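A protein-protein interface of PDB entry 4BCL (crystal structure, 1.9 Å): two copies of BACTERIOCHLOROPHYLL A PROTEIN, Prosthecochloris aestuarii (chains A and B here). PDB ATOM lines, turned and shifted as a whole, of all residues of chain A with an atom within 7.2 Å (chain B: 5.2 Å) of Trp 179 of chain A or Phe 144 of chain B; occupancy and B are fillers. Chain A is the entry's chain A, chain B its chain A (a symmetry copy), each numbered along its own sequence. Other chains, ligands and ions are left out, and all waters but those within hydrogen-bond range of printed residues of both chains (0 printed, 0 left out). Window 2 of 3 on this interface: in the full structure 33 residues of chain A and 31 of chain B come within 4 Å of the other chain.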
ATOM      1  N   GLY A 173     -12.128   0.063 -13.624  1.00  0.00           N
ATOM      2  CA  GLY A 173     -13.096  -1.050 -13.780  1.00  0.00           C
ATOM      3  C   GLY A 173     -12.812  -2.201 -12.822  1.00  0.00           C
ATOM      4  O   GLY A 173     -13.451  -2.317 -11.770  1.00  0.00           O
ATOM      5  N   ALA A 174     -11.821  -3.022 -13.179  1.00  0.00           N
ATOM      6  CA  ALA A 174     -11.261  -4.077 -12.324  1.00  0.00           C
ATOM      7  C   ALA A 174     -10.118  -3.440 -11.560  1.00  0.00           C
ATOM      8  O   ALA A 174      -9.723  -3.839 -10.471  1.00  0.00           O
ATOM      9  CB  ALA A 174     -10.673  -5.218 -13.128  1.00  0.00           C
ATOM     10  N   ASN A 175      -9.626  -2.350 -12.158  1.00  0.00           N
ATOM     11  CA  ASN A 175      -8.568  -1.570 -11.586  1.00  0.00           C
ATOM     12  C   ASN A 175      -8.984  -0.853 -10.361  1.00  0.00           C
ATOM     13  O   ASN A 175      -8.162  -0.614  -9.545  1.00  0.00           O
ATOM     14  CB  ASN A 175      -8.220  -0.529 -12.626  1.00  0.00           C
ATOM     15  CG  ASN A 175      -7.542  -1.201 -13.797  1.00  0.00           C
ATOM     16  OD1 ASN A 175      -6.801  -2.220 -13.655  1.00  0.00           O
ATOM     17  ND2 ASN A 175      -7.723  -0.530 -14.924  1.00  0.00           N
ATOM     18  N   PHE A 176     -10.244  -0.453 -10.329  1.00  0.00           N
ATOM     19  CA  PHE A 176     -10.717   0.292  -9.229  1.00  0.00           C
ATOM     20  C   PHE A 176     -10.342  -0.274  -7.875  1.00  0.00           C
ATOM     21  O   PHE A 176      -9.731   0.414  -7.047  1.00  0.00           O
ATOM     22  CB  PHE A 176     -12.157   0.799  -9.378  1.00  0.00           C
ATOM     23  CG  PHE A 176     -12.716   1.463  -8.091  1.00  0.00           C
ATOM     24  CD1 PHE A 176     -13.230   0.666  -7.060  1.00  0.00           C
ATOM     25  CD2 PHE A 176     -12.565   2.817  -7.787  1.00  0.00           C
ATOM     26  CE1 PHE A 176     -13.635   1.191  -5.824  1.00  0.00           C
ATOM     27  CE2 PHE A 176     -13.003   3.370  -6.586  1.00  0.00           C
ATOM     28  CZ  PHE A 176     -13.566   2.564  -5.593  1.00  0.00           C
ATOM     29  N   GLY A 177     -10.705  -1.523  -7.629  1.00  0.00           N
ATOM     30  CA  GLY A 177     -10.484  -2.081  -6.321  1.00  0.00           C
ATOM     31  C   GLY A 177      -9.031  -2.489  -6.054  1.00  0.00           C
ATOM     32  O   GLY A 177      -8.667  -2.882  -4.930  1.00  0.00           O
ATOM     33  N   ASP A 178      -8.266  -2.425  -7.148  1.00  0.00           N
ATOM     34  CA  ASP A 178      -6.862  -2.747  -7.054  1.00  0.00           C
ATOM     35  C   ASP A 178      -6.095  -1.440  -6.707  1.00  0.00           C
ATOM     36  O   ASP A 178      -5.520  -1.266  -5.631  1.00  0.00           O
ATOM     37  CB  ASP A 178      -6.414  -3.247  -8.391  1.00  0.00           C
ATOM     38  CG  ASP A 178      -4.929  -3.319  -8.575  1.00  0.00           C
ATOM     39  OD1 ASP A 178      -4.263  -3.123  -7.485  1.00  0.00           O
ATOM     40  OD2 ASP A 178      -4.422  -3.698  -9.601  1.00  0.00           O
ATOM     41  N   TRP A 179      -6.244  -0.481  -7.569  1.00  0.00           N
ATOM     42  CA  TRP A 179      -5.623   0.790  -7.440  1.00  0.00           C
ATOM     43  C   TRP A 179      -6.078   1.572  -6.243  1.00  0.00           C
ATOM     44  O   TRP A 179      -5.502   2.580  -5.875  1.00  0.00           O
ATOM     45  CB  TRP A 179      -5.872   1.589  -8.740  1.00  0.00           C
ATOM     46  CG  TRP A 179      -5.220   1.036  -9.964  1.00  0.00           C
ATOM     47  CD1 TRP A 179      -4.415  -0.043 -10.088  1.00  0.00           C
ATOM     48  CD2 TRP A 179      -5.423   1.565 -11.281  1.00  0.00           C
ATOM     49  NE1 TRP A 179      -4.162  -0.284 -11.434  1.00  0.00           N
ATOM     50  CE2 TRP A 179      -4.779   0.712 -12.182  1.00  0.00           C
ATOM     51  CE3 TRP A 179      -6.127   2.695 -11.742  1.00  0.00           C
ATOM     52  CZ2 TRP A 179      -4.695   1.045 -13.549  1.00  0.00           C
ATOM     53  CZ3 TRP A 179      -6.131   2.943 -13.102  1.00  0.00           C
ATOM     54  CH2 TRP A 179      -5.357   2.177 -13.957  1.00  0.00           C
ATOM     55  N   ILE A 180      -7.197   1.215  -5.675  1.00  0.00           N
ATOM     56  CA  ILE A 180      -7.632   2.051  -4.589  1.00  0.00           C
ATOM     57  C   ILE A 180      -6.613   1.969  -3.423  1.00  0.00           C
ATOM     58  O   ILE A 180      -6.538   2.791  -2.472  1.00  0.00           O
ATOM     59  CB  ILE A 180      -9.079   1.672  -4.151  1.00  0.00           C
ATOM     60  CG1 ILE A 180      -9.783   2.588  -3.148  1.00  0.00           C
ATOM     61  CG2 ILE A 180      -9.080   0.276  -3.457  1.00  0.00           C
ATOM     62  CD1 ILE A 180     -10.136   3.923  -3.733  1.00  0.00           C
ATOM     63  N   ARG A 181      -5.909   0.872  -3.413  1.00  0.00           N
ATOM     64  CA  ARG A 181      -5.017   0.634  -2.312  1.00  0.00           C
ATOM     65  C   ARG A 181      -3.985   1.751  -2.093  1.00  0.00           C
ATOM     66  O   ARG A 181      -3.718   2.085  -0.921  1.00  0.00           O
ATOM     67  CB  ARG A 181      -4.407  -0.793  -2.387  1.00  0.00           C
ATOM     68  CG  ARG A 181      -5.460  -1.883  -2.023  1.00  0.00           C
ATOM     69  CD  ARG A 181      -5.047  -3.327  -2.264  1.00  0.00           C
ATOM     70  NE  ARG A 181      -4.790  -3.420  -3.686  1.00  0.00           N
ATOM     71  CZ  ARG A 181      -4.324  -4.535  -4.120  1.00  0.00           C
ATOM     72  NH1 ARG A 181      -4.128  -5.473  -3.209  1.00  0.00           N
ATOM     73  NH2 ARG A 181      -4.069  -4.698  -5.416  1.00  0.00           N
ATOM     74  N   GLU A 182      -3.452   2.335  -3.211  1.00  0.00           N
ATOM     75  CA  GLU A 182      -2.413   3.377  -3.019  1.00  0.00           C
ATOM     76  C   GLU A 182      -3.111   4.622  -2.619  1.00  0.00           C
ATOM     77  O   GLU A 182      -2.512   5.574  -2.201  1.00  0.00           O
ATOM     78  CB  GLU A 182      -1.574   3.480  -4.308  1.00  0.00           C
ATOM     79  CG  GLU A 182      -2.427   3.769  -5.569  1.00  0.00           C
ATOM     80  CD  GLU A 182      -2.480   2.480  -6.326  1.00  0.00           C
ATOM     81  OE1 GLU A 182      -2.421   1.435  -5.730  1.00  0.00           O
ATOM     82  OE2 GLU A 182      -2.369   2.603  -7.633  1.00  0.00           O
ATOM     83  N   PHE A 183      -4.431   4.628  -2.806  1.00  0.00           N
ATOM     84  CA  PHE A 183      -5.087   5.840  -2.358  1.00  0.00           C
ATOM     85  C   PHE A 183      -5.333   5.759  -0.850  1.00  0.00           C
ATOM     86  O   PHE A 183      -5.174   6.718  -0.083  1.00  0.00           O
ATOM     87  CB  PHE A 183      -6.420   5.964  -3.155  1.00  0.00           C
ATOM     88  CG  PHE A 183      -7.280   7.051  -2.544  1.00  0.00           C
ATOM     89  CD1 PHE A 183      -7.059   8.384  -2.914  1.00  0.00           C
ATOM     90  CD2 PHE A 183      -8.308   6.727  -1.660  1.00  0.00           C
ATOM     91  CE1 PHE A 183      -7.830   9.428  -2.397  1.00  0.00           C
ATOM     92  CE2 PHE A 183      -9.110   7.758  -1.164  1.00  0.00           C
ATOM     93  CZ  PHE A 183      -8.906   9.085  -1.571  1.00  0.00           C
ATOM     94  N   TRP A 184      -5.789   4.575  -0.421  1.00  0.00           N
ATOM     95  CA  TRP A 184      -6.181   4.311   0.939  1.00  0.00           C
ATOM     96  C   TRP A 184      -5.012   4.334   1.911  1.00  0.00           C
ATOM     97  O   TRP A 184      -5.062   4.912   2.992  1.00  0.00           O
ATOM     98  CB  TRP A 184      -6.719   2.892   0.788  1.00  0.00           C
ATOM     99  CG  TRP A 184      -7.252   2.255   2.016  1.00  0.00           C
ATOM    100  CD1 TRP A 184      -7.194   2.647   3.332  1.00  0.00           C
ATOM    101  CD2 TRP A 184      -7.726   0.930   2.009  1.00  0.00           C
ATOM    102  NE1 TRP A 184      -7.743   1.654   4.130  1.00  0.00           N
ATOM    103  CE2 TRP A 184      -8.114   0.622   3.322  1.00  0.00           C
ATOM    104  CE3 TRP A 184      -7.922   0.037   0.935  1.00  0.00           C
ATOM    105  CZ2 TRP A 184      -8.596  -0.625   3.635  1.00  0.00           C
ATOM    106  CZ3 TRP A 184      -8.475  -1.179   1.242  1.00  0.00           C
ATOM    107  CH2 TRP A 184      -8.766  -1.485   2.568  1.00  0.00           C
ATOM    108  N   PRO A 202      -7.704  -6.597  -2.943  1.00  0.00           N
ATOM    109  CA  PRO A 202      -8.437  -5.561  -3.656  1.00  0.00           C
ATOM    110  C   PRO A 202      -9.829  -5.509  -3.024  1.00  0.00           C
ATOM    111  O   PRO A 202     -10.338  -6.382  -2.332  1.00  0.00           O
ATOM    112  CB  PRO A 202      -8.626  -6.042  -5.054  1.00  0.00           C
ATOM    113  CG  PRO A 202      -7.518  -7.054  -5.168  1.00  0.00           C
ATOM    114  CD  PRO A 202      -7.428  -7.731  -3.818  1.00  0.00           C
ATOM    115  N   SER B 117       4.638   9.824 -24.471  1.00  0.00           N
ATOM    116  CA  SER B 117       3.689  10.649 -23.791  1.00  0.00           C
ATOM    117  C   SER B 117       3.507  10.111 -22.338  1.00  0.00           C
ATOM    118  O   SER B 117       3.520   8.907 -22.046  1.00  0.00           O
ATOM    119  CB  SER B 117       2.393  10.393 -24.574  1.00  0.00           C
ATOM    120  OG  SER B 117       1.260  10.838 -23.847  1.00  0.00           O
ATOM    121  N   VAL B 118       3.255  11.052 -21.410  1.00  0.00           N
ATOM    122  CA  VAL B 118       3.051  10.713 -20.032  1.00  0.00           C
ATOM    123  C   VAL B 118       1.910  11.568 -19.547  1.00  0.00           C
ATOM    124  O   VAL B 118       1.890  12.797 -19.669  1.00  0.00           O
ATOM    125  CB  VAL B 118       4.325  10.892 -19.142  1.00  0.00           C
ATOM    126  CG1 VAL B 118       4.046  10.626 -17.640  1.00  0.00           C
ATOM    127  CG2 VAL B 118       5.496  10.071 -19.659  1.00  0.00           C
ATOM    128  N   VAL B 119       1.048  10.843 -18.934  1.00  0.00           N
ATOM    129  CA  VAL B 119      -0.150  11.350 -18.314  1.00  0.00           C
ATOM    130  C   VAL B 119      -0.182  11.093 -16.840  1.00  0.00           C
ATOM    131  O   VAL B 119      -0.127   9.938 -16.342  1.00  0.00           O
ATOM    132  CB  VAL B 119      -1.368  10.689 -18.975  1.00  0.00           C
ATOM    133  CG1 VAL B 119      -2.608  11.335 -18.373  1.00  0.00           C
ATOM    134  CG2 VAL B 119      -1.372  11.115 -20.448  1.00  0.00           C
ATOM    135  N   ASN B 120      -0.341  12.204 -16.128  1.00  0.00           N
ATOM    136  CA  ASN B 120      -0.381  12.047 -14.707  1.00  0.00           C
ATOM    137  C   ASN B 120      -1.781  12.171 -14.211  1.00  0.00           C
ATOM    138  O   ASN B 120      -2.523  13.087 -14.481  1.00  0.00           O
ATOM    139  CB  ASN B 120       0.443  13.189 -14.029  1.00  0.00           C
ATOM    140  CG  ASN B 120       0.696  12.872 -12.550  1.00  0.00           C
ATOM    141  OD1 ASN B 120       1.434  11.932 -12.210  1.00  0.00           O
ATOM    142  ND2 ASN B 120       0.097  13.664 -11.676  1.00  0.00           N
ATOM    143  N   MET B 121      -2.126  11.288 -13.337  1.00  0.00           N
ATOM    144  CA  MET B 121      -3.439  11.405 -12.820  1.00  0.00           C
ATOM    145  C   MET B 121      -3.546  11.237 -11.312  1.00  0.00           C
ATOM    146  O   MET B 121      -3.352  10.156 -10.758  1.00  0.00           O
ATOM    147  CB  MET B 121      -4.199  10.237 -13.465  1.00  0.00           C
ATOM    148  CG  MET B 121      -5.610  10.086 -12.931  1.00  0.00           C
ATOM    149  SD  MET B 121      -6.455   8.689 -13.709  1.00  0.00           S
ATOM    150  CE  MET B 121      -6.285   7.510 -12.332  1.00  0.00           C
ATOM    151  N   TYR B 123      -5.591  10.710  -7.964  1.00  0.00           N
ATOM    152  CA  TYR B 123      -6.716   9.905  -7.622  1.00  0.00           C
ATOM    153  C   TYR B 123      -8.004  10.672  -7.286  1.00  0.00           C
ATOM    154  O   TYR B 123      -9.102  10.392  -7.798  1.00  0.00           O
ATOM    155  CB  TYR B 123      -6.396   8.806  -6.608  1.00  0.00           C
ATOM    156  CG  TYR B 123      -5.651   7.666  -7.201  1.00  0.00           C
ATOM    157  CD1 TYR B 123      -5.977   7.232  -8.479  1.00  0.00           C
ATOM    158  CD2 TYR B 123      -4.564   7.087  -6.568  1.00  0.00           C
ATOM    159  CE1 TYR B 123      -5.333   6.134  -9.044  1.00  0.00           C
ATOM    160  CE2 TYR B 123      -3.895   6.008  -7.144  1.00  0.00           C
ATOM    161  CZ  TYR B 123      -4.299   5.501  -8.379  1.00  0.00           C
ATOM    162  OH  TYR B 123      -3.674   4.427  -8.983  1.00  0.00           O
ATOM    163  N   ARG B 142      -1.576   8.067 -10.290  1.00  0.00           N
ATOM    164  CA  ARG B 142      -0.962   6.991 -11.135  1.00  0.00           C
ATOM    165  C   ARG B 142      -0.523   7.740 -12.373  1.00  0.00           C
ATOM    166  O   ARG B 142      -1.178   8.730 -12.691  1.00  0.00           O
ATOM    167  CB  ARG B 142      -2.022   5.849 -11.458  1.00  0.00           C
ATOM    168  CG  ARG B 142      -1.462   4.832 -12.421  1.00  0.00           C
ATOM    169  CD  ARG B 142      -2.422   3.643 -12.379  1.00  0.00           C
ATOM    170  NE  ARG B 142      -2.353   2.925 -11.115  1.00  0.00           N
ATOM    171  CZ  ARG B 142      -1.514   1.900 -10.928  1.00  0.00           C
ATOM    172  NH1 ARG B 142      -0.663   1.459 -11.863  1.00  0.00           N
ATOM    173  NH2 ARG B 142      -1.513   1.231  -9.778  1.00  0.00           N
ATOM    174  N   GLN B 143       0.533   7.314 -13.049  1.00  0.00           N
ATOM    175  CA  GLN B 143       1.017   8.148 -14.122  1.00  0.00           C
ATOM    176  C   GLN B 143       1.315   7.204 -15.254  1.00  0.00           C
ATOM    177  O   GLN B 143       2.070   6.248 -15.120  1.00  0.00           O
ATOM    178  CB  GLN B 143       2.335   8.704 -13.532  1.00  0.00           C
ATOM    179  CG  GLN B 143       3.089   9.581 -14.505  1.00  0.00           C
ATOM    180  CD  GLN B 143       4.192  10.264 -13.724  1.00  0.00           C
ATOM    181  OE1 GLN B 143       5.332   9.802 -13.875  1.00  0.00           O
ATOM    182  NE2 GLN B 143       3.879  11.359 -13.003  1.00  0.00           N
ATOM    183  N   PHE B 144       0.645   7.397 -16.369  1.00  0.00           N
ATOM    184  CA  PHE B 144       0.709   6.460 -17.489  1.00  0.00           C
ATOM    185  C   PHE B 144       1.750   6.756 -18.561  1.00  0.00           C
ATOM    186  O   PHE B 144       1.766   7.845 -19.068  1.00  0.00           O
ATOM    187  CB  PHE B 144      -0.694   6.459 -18.141  1.00  0.00           C
ATOM    188  CG  PHE B 144      -1.721   6.059 -17.117  1.00  0.00           C
ATOM    189  CD1 PHE B 144      -2.309   7.057 -16.335  1.00  0.00           C
ATOM    190  CD2 PHE B 144      -2.111   4.726 -16.953  1.00  0.00           C
ATOM    191  CE1 PHE B 144      -3.321   6.773 -15.415  1.00  0.00           C
ATOM    192  CE2 PHE B 144      -3.107   4.408 -16.025  1.00  0.00           C
ATOM    193  CZ  PHE B 144      -3.669   5.425 -15.254  1.00  0.00           C
ATOM    194  N   HIS B 145       2.597   5.832 -18.875  1.00  0.00           N
ATOM    195  CA  HIS B 145       3.584   6.135 -19.879  1.00  0.00           C
ATOM    196  C   HIS B 145       3.196   5.452 -21.169  1.00  0.00           C
ATOM    197  O   HIS B 145       2.813   4.269 -21.173  1.00  0.00           O
ATOM    198  CB  HIS B 145       4.980   5.568 -19.534  1.00  0.00           C
ATOM    199  CG  HIS B 145       5.791   6.405 -18.531  1.00  0.00           C
ATOM    200  ND1 HIS B 145       5.271   6.685 -17.276  1.00  0.00           N
ATOM    201  CD2 HIS B 145       7.067   6.933 -18.570  1.00  0.00           C
ATOM    202  CE1 HIS B 145       6.162   7.451 -16.648  1.00  0.00           C
ATOM    203  NE2 HIS B 145       7.289   7.556 -17.359  1.00  0.00           N
ATOM    204  N   ASP B 146       3.420   6.127 -22.265  1.00  0.00           N
ATOM    205  CA  ASP B 146       3.154   5.487 -23.576  1.00  0.00           C
ATOM    206  C   ASP B 146       4.424   5.741 -24.364  1.00  0.00           C
ATOM    207  O   ASP B 146       4.811   6.876 -24.480  1.00  0.00           O
ATOM    208  CB  ASP B 146       1.906   6.073 -24.294  1.00  0.00           C
ATOM    209  CG  ASP B 146       1.592   5.343 -25.577  1.00  0.00           C
ATOM    210  OD1 ASP B 146       2.192   4.377 -25.968  1.00  0.00           O
ATOM    211  OD2 ASP B 146       0.587   5.843 -26.214  1.00  0.00           O
ATOM    212  N   ARG B 199       4.326   1.792  -7.075  1.00  0.00           N
ATOM    213  CA  ARG B 199       3.982   0.469  -7.659  1.00  0.00           C
ATOM    214  C   ARG B 199       4.222   0.607  -9.130  1.00  0.00           C
ATOM    215  O   ARG B 199       3.919   1.676  -9.677  1.00  0.00           O
ATOM    216  CB  ARG B 199       2.470   0.235  -7.587  1.00  0.00           C
ATOM    217  CG  ARG B 199       1.917   0.228  -6.196  1.00  0.00           C
ATOM    218  CD  ARG B 199       0.406  -0.122  -6.234  1.00  0.00           C
ATOM    219  NE  ARG B 199       0.196  -1.461  -6.825  1.00  0.00           N
ATOM    220  CZ  ARG B 199      -1.013  -1.956  -6.985  1.00  0.00           C
ATOM    221  NH1 ARG B 199      -2.119  -1.292  -6.728  1.00  0.00           N
ATOM    222  NH2 ARG B 199      -1.187  -3.113  -7.529  1.00  0.00           N
ATOM    223  N   PHE B 225       3.256   1.450 -19.761  1.00  0.00           N
ATOM    224  CA  PHE B 225       3.201   0.989 -18.393  1.00  0.00           C
ATOM    225  C   PHE B 225       2.785   2.153 -17.548  1.00  0.00           C
ATOM    226  O   PHE B 225       2.770   3.294 -18.015  1.00  0.00           O
ATOM    227  CB  PHE B 225       4.551   0.448 -17.887  1.00  0.00           C
ATOM    228  CG  PHE B 225       5.549   1.563 -17.546  1.00  0.00           C
ATOM    229  CD1 PHE B 225       6.402   2.108 -18.513  1.00  0.00           C
ATOM    230  CD2 PHE B 225       5.588   2.035 -16.231  1.00  0.00           C
ATOM    231  CE1 PHE B 225       7.325   3.125 -18.218  1.00  0.00           C
ATOM    232  CE2 PHE B 225       6.434   3.109 -15.920  1.00  0.00           C
ATOM    233  CZ  PHE B 225       7.302   3.618 -16.905  1.00  0.00           C
ATOM    234  N   SER B 226       2.384   1.829 -16.329  1.00  0.00           N
ATOM    235  CA  SER B 226       2.045   2.908 -15.487  1.00  0.00           C
ATOM    236  C   SER B 226       2.776   2.696 -14.107  1.00  0.00           C
ATOM    237  O   SER B 226       3.173   1.573 -13.730  1.00  0.00           O
ATOM    238  CB  SER B 226       0.514   3.115 -15.298  1.00  0.00           C
ATOM    239  OG  SER B 226      -0.119   2.114 -14.437  1.00  0.00           O
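Of the 13 printed residues of chain A, 5 touch a printed residue of chain B.
Hydrophobic or aromatic side chains of chain A within 4 Å of the printed part of chain B: Trp 179 and Phe 183.
Printed residues of chain B that touch a printed residue of chain A: Tyr 123, Arg 142, Phe 144 and Arg 199.
No position is printed for both chains.
The backbone carbonyl oxygen of Met 121 of chain B is in hydrogen-bond range of the backbone NH of Arg 142 of chain B.
The side-chain hydroxyl (OG) of Ser 226 of chain B sits at hydrogen-bond distance from the guanidinium group (NH1) of Arg 142 of chain B (2.7 Å).
O of Val 119 of chain B lies within hydrogen-bond range of N of Phe 144 of chain B (2.7 Å).
The side-chain carboxylate (OD1) of Asp 178 of chain A lies within salt-bridge range of the guanidinium group (NH2) of Arg 181 of chain A (2.6 Å).
The side-chain hydroxyl (OH) of Tyr 123 of chain B is in hydrogen-bond range of the guanidinium group (NE) of Arg 142 of chain B, at 2.9 Å.
Among the printed residues, merely in contact across the chains: Trp 179 of chain A with Tyr 123 of chain B (3.6 Å), Trp 179 of chain A with Phe 144 of chain B (3.8 Å), Arg 181 of chain A with Arg 199 of chain B (3.9 Å) and Phe 183 of chain A with Tyr 123 of chain B (3.8 Å).
The indole nitrogen (NE1) of Trp 179 of chain A lies close to the guanidinium group (NH2) of Arg 142 of chain B (3.5 Å).
OD1 of Asp 178 of chain A lies within salt-bridge range of NH1 of Arg 199 of chain B, 2.9 Å away.
The side-chain carboxylate (OE1) of Glu 182 of chain A lies within salt-bridge range of the guanidinium group (NH1) of Arg 199 of chain B, at 2.9 Å.
OE2 of Glu 182 of chain A lies within salt-bridge range of NH2 of Arg 142 of chain B (2.7 Å).
The side-chain hydroxyl (OH) of Tyr 123 of chain B is in hydrogen-bond range of the side-chain carboxylate (OE2) of Glu 182 of chain A, at 2.6 Å.
Printed residues of chain B within 4 Å of Asp 178 of chain A: Arg 199.
Trp 179 of chain A touches just these residues of chain B: Tyr 123 (3.6 Å), Arg 142 (3.2 Å) and Phe 144 (3.8 Å).
Of the printed residues of chain B, Arg 181 of chain A touches Arg 199 (3.9 Å).
Gln 143 of chain B touches none of the printed residues of chain A.
Phe 144 of chain B touches just one residue of chain A: Trp 179 (3.8 Å).
The nearest residue of chain B that does not touch Trp 179 of chain A is Arg 199 of chain B (4.1 Å).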
